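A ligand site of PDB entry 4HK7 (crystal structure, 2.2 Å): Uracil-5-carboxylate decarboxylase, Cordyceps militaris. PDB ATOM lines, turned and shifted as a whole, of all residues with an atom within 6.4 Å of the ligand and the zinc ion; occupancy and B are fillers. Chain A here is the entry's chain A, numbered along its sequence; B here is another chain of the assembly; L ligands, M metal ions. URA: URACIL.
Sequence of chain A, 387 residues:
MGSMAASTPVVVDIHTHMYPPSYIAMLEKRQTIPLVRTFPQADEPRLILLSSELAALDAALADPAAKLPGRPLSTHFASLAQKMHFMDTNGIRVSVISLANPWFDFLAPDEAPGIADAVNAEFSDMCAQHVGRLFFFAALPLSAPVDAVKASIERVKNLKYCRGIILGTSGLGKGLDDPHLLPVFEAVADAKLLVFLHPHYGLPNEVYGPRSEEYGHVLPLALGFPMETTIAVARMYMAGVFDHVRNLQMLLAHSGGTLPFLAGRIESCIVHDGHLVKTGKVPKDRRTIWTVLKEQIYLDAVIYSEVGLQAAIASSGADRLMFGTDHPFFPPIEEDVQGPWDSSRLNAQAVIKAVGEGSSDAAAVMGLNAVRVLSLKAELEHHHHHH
The zinc ion is bound by the side-chain carboxylate of Asp 326, a ring nitrogen (NE2) of His 15, an oxygen (O4) of the ligand, a ring nitrogen (NE2) of His 198 and a ring nitrogen (NE2) of His 17. The zinc ion has five donor atoms within binding distance.
Leu 49 touches the ligand. Leu 221 touches the ligand (CD2 to N1, 3.5 Å). Phe 225 touches the ligand. Phe 329 touches the ligand. Phe 330 touches the ligand (CZ to C6, 3.9 Å). Hydrophobic or aromatic side chains that line the ligand: His 17, Leu 49, His 198, Leu 221, Phe 225, Phe 329 and Phe 330. Of the 22 residues printed, 10 come within 4 Å of the ligand.
Within 4 Å of the zinc ion: His 15, His 17, His 198 and Asp 326.
OH of Tyr 19 lies within hydrogen-bond range of O of Asn 101, 2.6 Å away. The backbone carbonyl oxygen (O) of Leu 221 sits at hydrogen-bond distance from the guanidinium group (NE) of Arg 265 of chain B (2.8 Å). NE2 of His 254 is in hydrogen-bond range of OD2 of Asp 326 (3.1 Å). A ring nitrogen (ND1) of His 200 is in hydrogen-bond range of the side-chain amide nitrogen (ND2) of Asn 101 (3.0 Å). The backbone NH of His 17 is in hydrogen-bond range of the backbone carbonyl oxygen of His 327 (2.7 Å).
The guanidinium group (NH2) of Arg 71 lies within hydrogen-bond range of an oxygen (O2) of the ligand (2.7 Å). The side-chain amide oxygen (OD1) of Asn 101 lies within hydrogen-bond range of a nitrogen (N3) of the ligand.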
ATOM      1  N   HIS A  15      -9.875  29.359 -28.564  1.00  0.00           N
ATOM      2  CA  HIS A  15     -10.344  27.975 -28.504  1.00  0.00           C
ATOM      3  C   HIS A  15     -11.587  27.925 -27.676  1.00  0.00           C
ATOM      4  O   HIS A  15     -11.527  27.747 -26.463  1.00  0.00           O
ATOM      5  CB  HIS A  15      -9.257  27.052 -27.951  1.00  0.00           C
ATOM      6  CG  HIS A  15      -9.595  25.585 -28.091  1.00  0.00           C
ATOM      7  ND1 HIS A  15      -8.642  24.637 -28.217  1.00  0.00           N
ATOM      8  CD2 HIS A  15     -10.818  24.924 -28.151  1.00  0.00           C
ATOM      9  CE1 HIS A  15      -9.234  23.432 -28.324  1.00  0.00           C
ATOM     10  NE2 HIS A  15     -10.562  23.608 -28.286  1.00  0.00           N
ATOM     11  N   THR A  16     -12.729  28.055 -28.334  1.00  0.00           N
ATOM     12  CA  THR A  16     -14.007  28.279 -27.654  1.00  0.00           C
ATOM     13  C   THR A  16     -15.129  28.007 -28.648  1.00  0.00           C
ATOM     14  O   THR A  16     -15.055  28.420 -29.824  1.00  0.00           O
ATOM     15  CB  THR A  16     -14.073  29.709 -27.041  1.00  0.00           C
ATOM     16  OG1 THR A  16     -15.388  29.994 -26.561  1.00  0.00           O
ATOM     17  CG2 THR A  16     -13.655  30.781 -28.045  1.00  0.00           C
ATOM     18  N   HIS A  17     -16.161  27.289 -28.205  1.00  0.00           N
ATOM     19  CA  HIS A  17     -17.150  26.721 -29.126  1.00  0.00           C
ATOM     20  C   HIS A  17     -18.590  27.060 -28.862  1.00  0.00           C
ATOM     21  O   HIS A  17     -18.973  27.499 -27.770  1.00  0.00           O
ATOM     22  CB  HIS A  17     -17.058  25.204 -29.117  1.00  0.00           C
ATOM     23  CG  HIS A  17     -15.663  24.671 -29.357  1.00  0.00           C
ATOM     24  ND1 HIS A  17     -15.078  24.703 -30.566  1.00  0.00           N
ATOM     25  CD2 HIS A  17     -14.773  24.050 -28.492  1.00  0.00           C
ATOM     26  CE1 HIS A  17     -13.856  24.142 -30.471  1.00  0.00           C
ATOM     27  NE2 HIS A  17     -13.679  23.737 -29.216  1.00  0.00           N
ATOM     28  N   TYR A  19     -22.680  25.354 -30.352  1.00  0.00           N
ATOM     29  CA  TYR A  19     -23.570  24.663 -31.288  1.00  0.00           C
ATOM     30  C   TYR A  19     -24.784  25.560 -31.555  1.00  0.00           C
ATOM     31  O   TYR A  19     -25.634  25.712 -30.673  1.00  0.00           O
ATOM     32  CB  TYR A  19     -24.081  23.345 -30.704  1.00  0.00           C
ATOM     33  CG  TYR A  19     -23.055  22.259 -30.493  1.00  0.00           C
ATOM     34  CD1 TYR A  19     -22.217  21.845 -31.521  1.00  0.00           C
ATOM     35  CD2 TYR A  19     -22.967  21.598 -29.270  1.00  0.00           C
ATOM     36  CE1 TYR A  19     -21.301  20.827 -31.338  1.00  0.00           C
ATOM     37  CE2 TYR A  19     -22.048  20.572 -29.061  1.00  0.00           C
ATOM     38  CZ  TYR A  19     -21.218  20.199 -30.106  1.00  0.00           C
ATOM     39  OH  TYR A  19     -20.300  19.194 -29.927  1.00  0.00           O
ATOM     40  N   LEU A  49     -21.391  12.548 -28.250  1.00  0.00           N
ATOM     41  CA  LEU A  49     -20.559  12.899 -29.410  1.00  0.00           C
ATOM     42  C   LEU A  49     -19.529  11.847 -29.788  1.00  0.00           C
ATOM     43  O   LEU A  49     -19.171  11.721 -30.966  1.00  0.00           O
ATOM     44  CB  LEU A  49     -19.816  14.209 -29.142  1.00  0.00           C
ATOM     45  CG  LEU A  49     -20.627  15.456 -28.777  1.00  0.00           C
ATOM     46  CD1 LEU A  49     -19.680  16.527 -28.250  1.00  0.00           C
ATOM     47  CD2 LEU A  49     -21.421  15.952 -29.981  1.00  0.00           C
ATOM     48  N   LEU A  50     -19.032  11.114 -28.789  1.00  0.00           N
ATOM     49  CA  LEU A  50     -17.831  10.301 -28.940  1.00  0.00           C
ATOM     50  C   LEU A  50     -18.122   8.811 -28.980  1.00  0.00           C
ATOM     51  O   LEU A  50     -19.058   8.330 -28.333  1.00  0.00           O
ATOM     52  CB  LEU A  50     -16.853  10.605 -27.804  1.00  0.00           C
ATOM     53  CG  LEU A  50     -16.613  12.080 -27.423  1.00  0.00           C
ATOM     54  CD1 LEU A  50     -15.956  12.188 -26.044  1.00  0.00           C
ATOM     55  CD2 LEU A  50     -15.824  12.838 -28.480  1.00  0.00           C
ATOM     56  N   ARG A  71     -22.474  13.761 -22.061  1.00  0.00           N
ATOM     57  CA  ARG A  71     -22.358  14.929 -21.178  1.00  0.00           C
ATOM     58  C   ARG A  71     -23.627  15.792 -21.228  1.00  0.00           C
ATOM     59  O   ARG A  71     -24.392  15.690 -22.196  1.00  0.00           O
ATOM     60  CB  ARG A  71     -21.116  15.744 -21.535  1.00  0.00           C
ATOM     61  CG  ARG A  71     -19.818  15.076 -21.124  1.00  0.00           C
ATOM     62  CD  ARG A  71     -18.623  15.686 -21.835  1.00  0.00           C
ATOM     63  NE  ARG A  71     -18.642  15.451 -23.278  1.00  0.00           N
ATOM     64  CZ  ARG A  71     -17.660  15.792 -24.110  1.00  0.00           C
ATOM     65  NH1 ARG A  71     -16.568  16.395 -23.640  1.00  0.00           N
ATOM     66  NH2 ARG A  71     -17.763  15.535 -25.410  1.00  0.00           N
ATOM     67  N   ALA A 100     -18.192  23.174 -32.579  1.00  0.00           N
ATOM     68  CA  ALA A 100     -17.472  22.095 -31.899  1.00  0.00           C
ATOM     69  C   ALA A 100     -17.557  20.822 -32.718  1.00  0.00           C
ATOM     70  O   ALA A 100     -18.403  20.689 -33.598  1.00  0.00           O
ATOM     71  CB  ALA A 100     -18.026  21.876 -30.494  1.00  0.00           C
ATOM     72  N   ASN A 101     -16.662  19.883 -32.423  1.00  0.00           N
ATOM     73  CA  ASN A 101     -16.713  18.544 -32.984  1.00  0.00           C
ATOM     74  C   ASN A 101     -18.109  17.937 -32.760  1.00  0.00           C
ATOM     75  O   ASN A 101     -18.732  18.187 -31.726  1.00  0.00           O
ATOM     76  CB  ASN A 101     -15.636  17.674 -32.326  1.00  0.00           C
ATOM     77  CG  ASN A 101     -15.719  17.679 -30.804  1.00  0.00           C
ATOM     78  OD1 ASN A 101     -15.499  18.712 -30.162  1.00  0.00           O
ATOM     79  ND2 ASN A 101     -16.022  16.522 -30.226  1.00  0.00           N
ATOM     80  N   PHE A 196      -7.496  25.894 -38.024  1.00  0.00           N
ATOM     81  CA  PHE A 196      -7.521  25.424 -36.655  1.00  0.00           C
ATOM     82  C   PHE A 196      -7.806  23.927 -36.690  1.00  0.00           C
ATOM     83  O   PHE A 196      -8.905  23.489 -37.025  1.00  0.00           O
ATOM     84  CB  PHE A 196      -8.564  26.226 -35.859  1.00  0.00           C
ATOM     85  CG  PHE A 196      -8.695  25.830 -34.415  1.00  0.00           C
ATOM     86  CD1 PHE A 196      -7.608  25.331 -33.699  1.00  0.00           C
ATOM     87  CD2 PHE A 196      -9.903  25.982 -33.769  1.00  0.00           C
ATOM     88  CE1 PHE A 196      -7.742  24.972 -32.361  1.00  0.00           C
ATOM     89  CE2 PHE A 196     -10.054  25.627 -32.429  1.00  0.00           C
ATOM     90  CZ  PHE A 196      -8.967  25.115 -31.732  1.00  0.00           C
ATOM     91  N   HIS A 198      -8.340  20.383 -34.963  1.00  0.00           N
ATOM     92  CA  HIS A 198      -9.017  20.026 -33.717  1.00  0.00           C
ATOM     93  C   HIS A 198      -9.398  18.554 -33.714  1.00  0.00           C
ATOM     94  O   HIS A 198      -9.896  18.040 -34.714  1.00  0.00           O
ATOM     95  CB  HIS A 198     -10.259  20.898 -33.561  1.00  0.00           C
ATOM     96  CG  HIS A 198     -10.914  20.785 -32.205  1.00  0.00           C
ATOM     97  ND1 HIS A 198     -11.641  19.714 -31.854  1.00  0.00           N
ATOM     98  CD2 HIS A 198     -10.929  21.658 -31.118  1.00  0.00           C
ATOM     99  CE1 HIS A 198     -12.114  19.881 -30.594  1.00  0.00           C
ATOM    100  NE2 HIS A 198     -11.668  21.070 -30.144  1.00  0.00           N
ATOM    101  N   PRO A 199      -9.172  17.872 -32.570  1.00  0.00           N
ATOM    102  CA  PRO A 199      -9.456  16.432 -32.508  1.00  0.00           C
ATOM    103  C   PRO A 199     -10.956  16.121 -32.368  1.00  0.00           C
ATOM    104  O   PRO A 199     -11.763  17.030 -32.172  1.00  0.00           O
ATOM    105  CB  PRO A 199      -8.737  16.007 -31.225  1.00  0.00           C
ATOM    106  CG  PRO A 199      -8.874  17.218 -30.349  1.00  0.00           C
ATOM    107  CD  PRO A 199      -8.656  18.381 -31.293  1.00  0.00           C
ATOM    108  N   HIS A 200     -11.302  14.840 -32.484  1.00  0.00           N
ATOM    109  CA  HIS A 200     -12.666  14.345 -32.240  1.00  0.00           C
ATOM    110  C   HIS A 200     -12.757  12.855 -32.175  1.00  0.00           C
ATOM    111  O   HIS A 200     -13.446  12.304 -31.307  1.00  0.00           O
ATOM    112  CB  HIS A 200     -13.643  14.813 -33.322  1.00  0.00           C
ATOM    113  CG  HIS A 200     -14.972  14.098 -33.261  1.00  0.00           C
ATOM    114  ND1 HIS A 200     -15.870  14.316 -32.275  1.00  0.00           N
ATOM    115  CD2 HIS A 200     -15.518  13.110 -34.072  1.00  0.00           C
ATOM    116  CE1 HIS A 200     -16.948  13.530 -32.465  1.00  0.00           C
ATOM    117  NE2 HIS A 200     -16.725  12.787 -33.559  1.00  0.00           N
ATOM    118  N   LEU A 221     -10.596  11.990 -23.305  1.00  0.00           N
ATOM    119  CA  LEU A 221     -10.389  13.440 -23.371  1.00  0.00           C
ATOM    120  C   LEU A 221      -8.973  13.886 -23.029  1.00  0.00           C
ATOM    121  O   LEU A 221      -8.431  14.789 -23.673  1.00  0.00           O
ATOM    122  CB  LEU A 221     -11.384  14.202 -22.481  1.00  0.00           C
ATOM    123  CG  LEU A 221     -12.869  14.151 -22.830  1.00  0.00           C
ATOM    124  CD1 LEU A 221     -13.662  14.952 -21.802  1.00  0.00           C
ATOM    125  CD2 LEU A 221     -13.141  14.658 -24.247  1.00  0.00           C
ATOM    126  N   PHE A 225      -7.759  12.593 -27.440  1.00  0.00           N
ATOM    127  CA  PHE A 225      -7.799  13.846 -28.199  1.00  0.00           C
ATOM    128  C   PHE A 225      -6.404  14.366 -28.624  1.00  0.00           C
ATOM    129  O   PHE A 225      -6.131  14.487 -29.814  1.00  0.00           O
ATOM    130  CB  PHE A 225      -8.571  14.918 -27.408  1.00  0.00           C
ATOM    131  CG  PHE A 225     -10.044  14.961 -27.680  1.00  0.00           C
ATOM    132  CD1 PHE A 225     -10.723  13.863 -28.213  1.00  0.00           C
ATOM    133  CD2 PHE A 225     -10.774  16.117 -27.408  1.00  0.00           C
ATOM    134  CE1 PHE A 225     -12.085  13.916 -28.472  1.00  0.00           C
ATOM    135  CE2 PHE A 225     -12.134  16.183 -27.671  1.00  0.00           C
ATOM    136  CZ  PHE A 225     -12.790  15.076 -28.201  1.00  0.00           C
ATOM    137  N   ALA A 253      -4.854  22.563 -31.744  1.00  0.00           N
ATOM    138  CA  ALA A 253      -5.539  22.452 -30.473  1.00  0.00           C
ATOM    139  C   ALA A 253      -4.670  21.765 -29.433  1.00  0.00           C
ATOM    140  O   ALA A 253      -3.882  20.867 -29.757  1.00  0.00           O
ATOM    141  CB  ALA A 253      -6.850  21.681 -30.650  1.00  0.00           C
ATOM    142  N   HIS A 254      -4.813  22.213 -28.187  1.00  0.00           N
ATOM    143  CA  HIS A 254      -4.171  21.578 -27.028  1.00  0.00           C
ATOM    144  C   HIS A 254      -2.679  21.548 -27.145  1.00  0.00           C
ATOM    145  O   HIS A 254      -2.038  20.502 -26.942  1.00  0.00           O
ATOM    146  CB  HIS A 254      -4.775  20.195 -26.800  1.00  0.00           C
ATOM    147  CG  HIS A 254      -6.284  20.180 -26.849  1.00  0.00           C
ATOM    148  ND1 HIS A 254      -6.986  19.327 -27.606  1.00  0.00           N
ATOM    149  CD2 HIS A 254      -7.215  21.004 -26.206  1.00  0.00           C
ATOM    150  CE1 HIS A 254      -8.298  19.556 -27.452  1.00  0.00           C
ATOM    151  NE2 HIS A 254      -8.437  20.591 -26.595  1.00  0.00           N
ATOM    152  N   ASP A 326     -11.374  26.313 -24.289  1.00  0.00           N
ATOM    153  CA  ASP A 326     -12.218  25.177 -24.654  1.00  0.00           C
ATOM    154  C   ASP A 326     -13.638  25.274 -24.076  1.00  0.00           C
ATOM    155  O   ASP A 326     -14.312  24.262 -23.884  1.00  0.00           O
ATOM    156  CB  ASP A 326     -11.571  23.838 -24.275  1.00  0.00           C
ATOM    157  CG  ASP A 326     -11.763  22.769 -25.344  1.00  0.00           C
ATOM    158  OD1 ASP A 326     -12.614  22.961 -26.236  1.00  0.00           O
ATOM    159  OD2 ASP A 326     -11.033  21.755 -25.296  1.00  0.00           O
ATOM    160  N   HIS A 327     -14.085  26.508 -23.803  1.00  0.00           N
ATOM    161  CA  HIS A 327     -15.477  26.751 -23.379  1.00  0.00           C
ATOM    162  C   HIS A 327     -16.396  26.205 -24.448  1.00  0.00           C
ATOM    163  O   HIS A 327     -16.106  26.379 -25.625  1.00  0.00           O
ATOM    164  CB  HIS A 327     -15.701  28.245 -23.175  1.00  0.00           C
ATOM    165  CG  HIS A 327     -17.085  28.585 -22.665  1.00  0.00           C
ATOM    166  ND1 HIS A 327     -18.047  29.067 -23.480  1.00  0.00           N
ATOM    167  CD2 HIS A 327     -17.642  28.498 -21.400  1.00  0.00           C
ATOM    168  CE1 HIS A 327     -19.173  29.281 -22.759  1.00  0.00           C
ATOM    169  NE2 HIS A 327     -18.919  28.925 -21.497  1.00  0.00           N
ATOM    170  N   PHE A 329     -16.806  23.189 -22.653  1.00  0.00           N
ATOM    171  CA  PHE A 329     -16.743  21.744 -22.429  1.00  0.00           C
ATOM    172  C   PHE A 329     -16.349  21.310 -21.004  1.00  0.00           C
ATOM    173  O   PHE A 329     -16.697  20.214 -20.596  1.00  0.00           O
ATOM    174  CB  PHE A 329     -15.875  21.044 -23.480  1.00  0.00           C
ATOM    175  CG  PHE A 329     -16.581  20.813 -24.793  1.00  0.00           C
ATOM    176  CD1 PHE A 329     -17.431  19.710 -24.963  1.00  0.00           C
ATOM    177  CD2 PHE A 329     -16.396  21.687 -25.859  1.00  0.00           C
ATOM    178  CE1 PHE A 329     -18.066  19.489 -26.177  1.00  0.00           C
ATOM    179  CE2 PHE A 329     -17.037  21.473 -27.078  1.00  0.00           C
ATOM    180  CZ  PHE A 329     -17.878  20.372 -27.234  1.00  0.00           C
ATOM    181  N   PHE A 330     -15.627  22.160 -20.272  1.00  0.00           N
ATOM    182  CA  PHE A 330     -15.262  21.798 -18.898  1.00  0.00           C
ATOM    183  C   PHE A 330     -15.802  22.778 -17.839  1.00  0.00           C
ATOM    184  O   PHE A 330     -15.033  23.557 -17.257  1.00  0.00           O
ATOM    185  CB  PHE A 330     -13.745  21.640 -18.773  1.00  0.00           C
ATOM    186  CG  PHE A 330     -13.143  20.667 -19.748  1.00  0.00           C
ATOM    187  CD1 PHE A 330     -13.102  19.310 -19.461  1.00  0.00           C
ATOM    188  CD2 PHE A 330     -12.608  21.115 -20.954  1.00  0.00           C
ATOM    189  CE1 PHE A 330     -12.547  18.408 -20.367  1.00  0.00           C
ATOM    190  CE2 PHE A 330     -12.046  20.220 -21.859  1.00  0.00           C
ATOM    191  CZ  PHE A 330     -12.013  18.869 -21.554  1.00  0.00           C
ATOM    192  N   ARG B 265      -3.230  18.262 -18.246  1.00  0.00           N
ATOM    193  CA  ARG B 265      -4.482  17.911 -18.903  1.00  0.00           C
ATOM    194  C   ARG B 265      -5.225  16.768 -18.187  1.00  0.00           C
ATOM    195  O   ARG B 265      -6.460  16.807 -18.035  1.00  0.00           O
ATOM    196  CB  ARG B 265      -4.251  17.555 -20.383  1.00  0.00           C
ATOM    197  CG  ARG B 265      -5.544  17.439 -21.176  1.00  0.00           C
ATOM    198  CD  ARG B 265      -5.341  16.954 -22.602  1.00  0.00           C
ATOM    199  NE  ARG B 265      -6.637  16.833 -23.255  1.00  0.00           N
ATOM    200  CZ  ARG B 265      -7.394  17.871 -23.626  1.00  0.00           C
ATOM    201  NH1 ARG B 265      -6.965  19.123 -23.438  1.00  0.00           N
ATOM    202  NH2 ARG B 265      -8.579  17.671 -24.188  1.00  0.00           N
HETATM  203  N1  URA L   1     -14.803  17.500 -25.348  1.00  0.00           N
HETATM  204  C2  URA L   1     -15.241  17.548 -26.692  1.00  0.00           C
HETATM  205  O2  URA L   1     -15.967  16.671 -27.150  1.00  0.00           O
HETATM  206  N3  URA L   1     -14.817  18.597 -27.511  1.00  0.00           N
HETATM  207  C4  URA L   1     -13.982  19.582 -26.982  1.00  0.00           C
HETATM  208  O4  URA L   1     -13.623  20.520 -27.701  1.00  0.00           O
HETATM  209  C5  URA L   1     -13.574  19.507 -25.643  1.00  0.00           C
HETATM  210  C6  URA L   1     -14.010  18.446 -24.847  1.00  0.00           C
HETATM  211 ZN    ZN M   1     -12.243  22.163 -28.260  1.00  0.00          ZN
